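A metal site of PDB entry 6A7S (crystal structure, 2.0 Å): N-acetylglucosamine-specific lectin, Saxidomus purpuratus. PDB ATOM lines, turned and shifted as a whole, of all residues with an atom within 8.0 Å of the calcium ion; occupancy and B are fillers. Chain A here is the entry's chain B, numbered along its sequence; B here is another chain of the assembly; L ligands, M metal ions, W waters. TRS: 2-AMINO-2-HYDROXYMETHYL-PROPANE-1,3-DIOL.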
ATOM      1  N   PHE A  35       6.575  -2.609  29.128  1.00  0.00           N
ATOM      2  CA  PHE A  35       6.229  -1.209  29.271  1.00  0.00           C
ATOM      3  C   PHE A  35       5.491  -0.745  28.029  1.00  0.00           C
ATOM      4  O   PHE A  35       5.981  -0.889  26.921  1.00  0.00           O
ATOM      5  CB  PHE A  35       7.459  -0.297  29.438  1.00  0.00           C
ATOM      6  CG  PHE A  35       7.096   1.168  29.382  1.00  0.00           C
ATOM      7  CD1 PHE A  35       6.627   1.804  30.515  1.00  0.00           C
ATOM      8  CD2 PHE A  35       7.091   1.855  28.176  1.00  0.00           C
ATOM      9  CE1 PHE A  35       6.197   3.115  30.470  1.00  0.00           C
ATOM     10  CE2 PHE A  35       6.648   3.183  28.123  1.00  0.00           C
ATOM     11  CZ  PHE A  35       6.245   3.816  29.282  1.00  0.00           C
ATOM     12  N   GLY A  36       4.325  -0.106  28.232  1.00  0.00           N
ATOM     13  CA  GLY A  36       3.775   0.761  27.196  1.00  0.00           C
ATOM     14  C   GLY A  36       3.437   0.044  25.911  1.00  0.00           C
ATOM     15  O   GLY A  36       3.534   0.636  24.824  1.00  0.00           O
ATOM     16  N   GLY A  37       3.025  -1.218  26.036  1.00  0.00           N
ATOM     17  CA  GLY A  37       2.633  -1.983  24.885  1.00  0.00           C
ATOM     18  C   GLY A  37       3.780  -2.692  24.197  1.00  0.00           C
ATOM     19  O   GLY A  37       3.562  -3.315  23.134  1.00  0.00           O
ATOM     20  N   SER A  38       4.993  -2.660  24.803  1.00  0.00           N
ATOM     21  CA  SER A  38       6.151  -3.326  24.246  1.00  0.00           C
ATOM     22  C   SER A  38       6.768  -4.256  25.306  1.00  0.00           C
ATOM     23  O   SER A  38       6.550  -4.073  26.518  1.00  0.00           O
ATOM     24  CB  SER A  38       7.143  -2.343  23.720  1.00  0.00           C
ATOM     25  OG  SER A  38       6.796  -1.871  22.456  1.00  0.00           O
ATOM     26  N   CYS A  39       7.479  -5.289  24.824  1.00  0.00           N
ATOM     27  CA  CYS A  39       8.328  -6.098  25.680  1.00  0.00           C
ATOM     28  C   CYS A  39       9.795  -5.783  25.335  1.00  0.00           C
ATOM     29  O   CYS A  39      10.151  -5.586  24.175  1.00  0.00           O
ATOM     30  CB  CYS A  39       8.016  -7.578  25.521  1.00  0.00           C
ATOM     31  SG  CYS A  39       6.342  -7.988  26.086  1.00  0.00           S
ATOM     32  N   TYR A  40      10.633  -5.697  26.368  1.00  0.00           N
ATOM     33  CA  TYR A  40      12.042  -5.198  26.226  1.00  0.00           C
ATOM     34  C   TYR A  40      12.998  -6.231  26.798  1.00  0.00           C
ATOM     35  O   TYR A  40      12.752  -6.867  27.842  1.00  0.00           O
ATOM     36  CB  TYR A  40      12.207  -3.883  26.990  1.00  0.00           C
ATOM     37  CG  TYR A  40      11.331  -2.768  26.482  1.00  0.00           C
ATOM     38  CD1 TYR A  40      10.051  -2.568  26.978  1.00  0.00           C
ATOM     39  CD2 TYR A  40      11.780  -1.896  25.526  1.00  0.00           C
ATOM     40  CE1 TYR A  40       9.228  -1.576  26.489  1.00  0.00           C
ATOM     41  CE2 TYR A  40      10.999  -0.861  25.075  1.00  0.00           C
ATOM     42  CZ  TYR A  40       9.710  -0.684  25.549  1.00  0.00           C
ATOM     43  OH  TYR A  40       8.896   0.323  25.024  1.00  0.00           O
ATOM     44  N   LEU A  63      16.434  -3.933  17.679  1.00  0.00           N
ATOM     45  CA  LEU A  63      16.951  -2.911  18.643  1.00  0.00           C
ATOM     46  C   LEU A  63      15.845  -1.889  18.892  1.00  0.00           C
ATOM     47  O   LEU A  63      15.146  -1.476  17.937  1.00  0.00           O
ATOM     48  CB  LEU A  63      18.157  -2.207  18.047  1.00  0.00           C
ATOM     49  CG  LEU A  63      19.481  -2.947  18.152  1.00  0.00           C
ATOM     50  CD1 LEU A  63      20.552  -2.304  17.279  1.00  0.00           C
ATOM     51  CD2 LEU A  63      19.937  -3.103  19.592  1.00  0.00           C
ATOM     52  N   VAL A  64      15.755  -1.428  20.146  1.00  0.00           N
ATOM     53  CA  VAL A  64      14.683  -0.580  20.643  1.00  0.00           C
ATOM     54  C   VAL A  64      14.580   0.709  19.829  1.00  0.00           C
ATOM     55  O   VAL A  64      15.571   1.273  19.369  1.00  0.00           O
ATOM     56  CB  VAL A  64      14.842  -0.273  22.129  1.00  0.00           C
ATOM     57  CG1 VAL A  64      16.009   0.701  22.316  1.00  0.00           C
ATOM     58  CG2 VAL A  64      13.547   0.263  22.712  1.00  0.00           C
ATOM     59  N   THR A  65      13.320   1.143  19.585  1.00  0.00           N
ATOM     60  CA  THR A  65      13.011   2.461  18.987  1.00  0.00           C
ATOM     61  C   THR A  65      12.221   3.230  20.029  1.00  0.00           C
ATOM     62  O   THR A  65      11.414   2.660  20.775  1.00  0.00           O
ATOM     63  CB  THR A  65      12.315   2.366  17.609  1.00  0.00           C
ATOM     64  OG1 THR A  65      11.008   1.797  17.781  1.00  0.00           O
ATOM     65  CG2 THR A  65      13.128   1.555  16.623  1.00  0.00           C
ATOM     66  N   VAL A  66      12.509   4.534  20.144  1.00  0.00           N
ATOM     67  CA  VAL A  66      11.992   5.270  21.261  1.00  0.00           C
ATOM     68  C   VAL A  66      11.060   6.382  20.771  1.00  0.00           C
ATOM     69  O   VAL A  66      11.523   7.441  20.291  1.00  0.00           O
ATOM     70  CB  VAL A  66      13.092   5.789  22.200  1.00  0.00           C
ATOM     71  CG1 VAL A  66      12.505   6.398  23.459  1.00  0.00           C
ATOM     72  CG2 VAL A  66      14.065   4.691  22.584  1.00  0.00           C
ATOM     73  N   GLU A  67       9.735   6.122  20.863  1.00  0.00           N
ATOM     74  CA  GLU A  67       8.733   6.990  20.215  1.00  0.00           C
ATOM     75  C   GLU A  67       8.270   8.082  21.167  1.00  0.00           C
ATOM     76  O   GLU A  67       7.607   9.008  20.713  1.00  0.00           O
ATOM     77  CB  GLU A  67       7.495   6.226  19.752  1.00  0.00           C
ATOM     78  CG  GLU A  67       7.770   5.364  18.525  1.00  0.00           C
ATOM     79  CD  GLU A  67       8.553   4.085  18.736  1.00  0.00           C
ATOM     80  OE1 GLU A  67       8.593   3.502  19.915  1.00  0.00           O
ATOM     81  OE2 GLU A  67       9.160   3.649  17.750  1.00  0.00           O
ATOM     82  N   CYS A  68       8.586   7.982  22.463  1.00  0.00           N
ATOM     83  CA  CYS A  68       7.992   8.961  23.360  1.00  0.00           C
ATOM     84  C   CYS A  68       8.742   9.078  24.693  1.00  0.00           C
ATOM     85  O   CYS A  68       9.505   8.198  25.069  1.00  0.00           O
ATOM     86  CB  CYS A  68       6.573   8.554  23.657  1.00  0.00           C
ATOM     87  SG  CYS A  68       6.584   6.922  24.411  1.00  0.00           S
ATOM     88  N   GLU A  71       8.614   6.284  27.333  1.00  0.00           N
ATOM     89  CA  GLU A  71       9.417   5.142  26.985  1.00  0.00           C
ATOM     90  C   GLU A  71      10.902   5.484  27.219  1.00  0.00           C
ATOM     91  O   GLU A  71      11.615   4.701  27.709  1.00  0.00           O
ATOM     92  CB  GLU A  71       9.233   4.774  25.513  1.00  0.00           C
ATOM     93  CG  GLU A  71       9.901   3.456  25.095  1.00  0.00           C
ATOM     94  CD  GLU A  71       9.647   3.038  23.641  1.00  0.00           C
ATOM     95  OE1 GLU A  71       9.365   3.899  22.790  1.00  0.00           O
ATOM     96  OE2 GLU A  71       9.782   1.857  23.346  1.00  0.00           O
ATOM     97  N   ASP A  72      11.322   6.654  26.794  1.00  0.00           N
ATOM     98  CA  ASP A  72      12.657   7.132  27.134  1.00  0.00           C
ATOM     99  C   ASP A  72      12.898   7.012  28.646  1.00  0.00           C
ATOM    100  O   ASP A  72      13.971   6.550  29.120  1.00  0.00           O
ATOM    101  CB  ASP A  72      12.812   8.546  26.599  1.00  0.00           C
ATOM    102  CG  ASP A  72      14.141   9.197  26.961  1.00  0.00           C
ATOM    103  OD1 ASP A  72      15.123   8.859  26.315  1.00  0.00           O
ATOM    104  OD2 ASP A  72      14.139  10.058  27.878  1.00  0.00           O
ATOM    105  N   ILE A  75      13.188   3.376  29.981  1.00  0.00           N
ATOM    106  CA  ILE A  75      14.514   2.884  29.689  1.00  0.00           C
ATOM    107  C   ILE A  75      15.520   3.487  30.682  1.00  0.00           C
ATOM    108  O   ILE A  75      16.356   2.760  31.236  1.00  0.00           O
ATOM    109  CB  ILE A  75      14.896   3.206  28.244  1.00  0.00           C
ATOM    110  CG1 ILE A  75      14.139   2.309  27.248  1.00  0.00           C
ATOM    111  CG2 ILE A  75      16.388   3.090  28.042  1.00  0.00           C
ATOM    112  CD1 ILE A  75      14.217   2.856  25.852  1.00  0.00           C
ATOM    113  N   TRP A 103      15.246   5.969  13.083  1.00  0.00           N
ATOM    114  CA  TRP A 103      15.114   4.608  13.523  1.00  0.00           C
ATOM    115  C   TRP A 103      15.431   3.664  12.363  1.00  0.00           C
ATOM    116  O   TRP A 103      15.311   4.020  11.184  1.00  0.00           O
ATOM    117  CB  TRP A 103      13.741   4.366  14.141  1.00  0.00           C
ATOM    118  CG  TRP A 103      13.466   5.302  15.275  1.00  0.00           C
ATOM    119  CD1 TRP A 103      12.473   6.247  15.333  1.00  0.00           C
ATOM    120  CD2 TRP A 103      14.180   5.387  16.521  1.00  0.00           C
ATOM    121  NE1 TRP A 103      12.558   6.931  16.521  1.00  0.00           N
ATOM    122  CE2 TRP A 103      13.608   6.441  17.265  1.00  0.00           C
ATOM    123  CE3 TRP A 103      15.290   4.717  17.053  1.00  0.00           C
ATOM    124  CZ2 TRP A 103      14.076   6.807  18.530  1.00  0.00           C
ATOM    125  CZ3 TRP A 103      15.747   5.073  18.301  1.00  0.00           C
ATOM    126  CH2 TRP A 103      15.167   6.121  19.019  1.00  0.00           C
ATOM    127  N   ASP A 105      13.833   1.154  11.612  1.00  0.00           N
ATOM    128  CA  ASP A 105      12.627   0.736  10.864  1.00  0.00           C
ATOM    129  C   ASP A 105      12.314   1.731   9.750  1.00  0.00           C
ATOM    130  O   ASP A 105      11.296   1.588   9.125  1.00  0.00           O
ATOM    131  CB  ASP A 105      11.375   0.541  11.729  1.00  0.00           C
ATOM    132  CG  ASP A 105      11.002   1.734  12.578  1.00  0.00           C
ATOM    133  OD1 ASP A 105      11.501   2.841  12.280  1.00  0.00           O
ATOM    134  OD2 ASP A 105      10.270   1.538  13.579  1.00  0.00           O
ATOM    135  N   GLU A 154      13.482  -4.834  21.446  1.00  0.00           N
ATOM    136  CA  GLU A 154      12.067  -4.511  21.660  1.00  0.00           C
ATOM    137  C   GLU A 154      11.217  -5.435  20.775  1.00  0.00           C
ATOM    138  O   GLU A 154      11.596  -5.609  19.617  1.00  0.00           O
ATOM    139  CB  GLU A 154      11.776  -3.059  21.253  1.00  0.00           C
ATOM    140  CG  GLU A 154      10.390  -2.545  21.672  1.00  0.00           C
ATOM    141  CD  GLU A 154      10.061  -1.111  21.303  1.00  0.00           C
ATOM    142  OE1 GLU A 154      10.845  -0.499  20.501  1.00  0.00           O
ATOM    143  OE2 GLU A 154       8.984  -0.615  21.768  1.00  0.00           O
ATOM    144  N   ILE A 155      10.082  -5.883  21.314  1.00  0.00           N
ATOM    145  CA  ILE A 155       8.951  -6.405  20.499  1.00  0.00           C
ATOM    146  C   ILE A 155       7.679  -5.649  20.866  1.00  0.00           C
ATOM    147  O   ILE A 155       7.432  -5.294  22.018  1.00  0.00           O
ATOM    148  CB  ILE A 155       8.765  -7.920  20.688  1.00  0.00           C
ATOM    149  CG1 ILE A 155       8.379  -8.305  22.118  1.00  0.00           C
ATOM    150  CG2 ILE A 155      10.014  -8.643  20.207  1.00  0.00           C
ATOM    151  CD1 ILE A 155       7.984  -9.785  22.325  1.00  0.00           C
ATOM    152  N   ASP A 156       6.800  -5.513  19.877  1.00  0.00           N
ATOM    153  CA  ASP A 156       5.487  -4.927  20.145  1.00  0.00           C
ATOM    154  C   ASP A 156       4.317  -5.874  19.824  1.00  0.00           C
ATOM    155  O   ASP A 156       3.197  -5.437  19.725  1.00  0.00           O
ATOM    156  CB  ASP A 156       5.393  -3.646  19.352  1.00  0.00           C
ATOM    157  CG  ASP A 156       5.248  -3.875  17.868  1.00  0.00           C
ATOM    158  OD1 ASP A 156       5.191  -5.048  17.463  1.00  0.00           O
ATOM    159  OD2 ASP A 156       5.193  -2.879  17.159  1.00  0.00           O
ATOM    160  N   CYS B  22       2.521   4.022  24.394  1.00  0.00           N
ATOM    161  CA  CYS B  22       3.419   4.338  25.478  1.00  0.00           C
ATOM    162  C   CYS B  22       2.610   4.463  26.755  1.00  0.00           C
ATOM    163  O   CYS B  22       3.157   4.746  27.818  1.00  0.00           O
ATOM    164  CB  CYS B  22       4.171   5.632  25.152  1.00  0.00           C
ATOM    165  SG  CYS B  22       5.104   5.482  23.608  1.00  0.00           S
HETATM  166  C   TRS L   1       8.895  -0.954  17.560  1.00  0.00           C
HETATM  167  C1  TRS L   1       8.399  -0.269  16.277  1.00  0.00           C
HETATM  168  C2  TRS L   1       8.801  -2.466  17.342  1.00  0.00           C
HETATM  169  C3  TRS L   1       8.051  -0.450  18.769  1.00  0.00           C
HETATM  170  N   TRS L   1      10.340  -0.594  17.779  1.00  0.00           N
HETATM  171  O1  TRS L   1       9.426  -0.475  15.330  1.00  0.00           O
HETATM  172  O2  TRS L   1       9.346  -3.165  18.454  1.00  0.00           O
HETATM  173  O3  TRS L   1       8.396   0.917  19.035  1.00  0.00           O
HETATM  174 CA    CA M   1       9.321   1.696  21.072  1.00  0.00          CA
HETATM  175  O   HOH W   1       6.993   1.844  21.922  1.00  0.00           O
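The backbone NH of Glu 71 sits close to the side-chain sulfur of Cys 68, 3.6 Å away.
OE2 of Glu 71 lies close to OH of Tyr 40, 2.4 Å away.
OE2 of Glu 154 lies close to OH of Tyr 40, 3.4 Å away.
The side-chain carboxylate (OE2) of Glu 154 lies close to the side-chain hydroxyl (OG) of Ser 38 (2.6 Å).
The side-chain sulfur (SG) of Cys 22 of chain B forms a disulfide with the side-chain sulfur (SG) of Cys 68.
The calcium ion is bound by the side-chain carboxylate (OE1) of Glu 67 (2.3 Å), the backbone carbonyl oxygen (O) of Thr 65 (2.3 Å), the side-chain carboxylate (OE2) of Glu 71 (2.3 Å), an oxygen (O3) of the ligand (2.4 Å), the side-chain carboxylate (OE2) of Glu 154 (2.4 Å), water W1 (2.5 Å), the side-chain carboxylate (OE1) of Glu 154 (2.7 Å) and the side-chain carboxylate (OE1) of Glu 71 (2.8 Å).
The calcium ion has eight donor atoms within binding distance.
Four residues have an atom within 4 Å of the calcium ion: Thr 65, Glu 67, Glu 71 and Glu 154.
The nearest printed residue that does not touch the calcium ion is Tyr 40 (4.2 Å).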
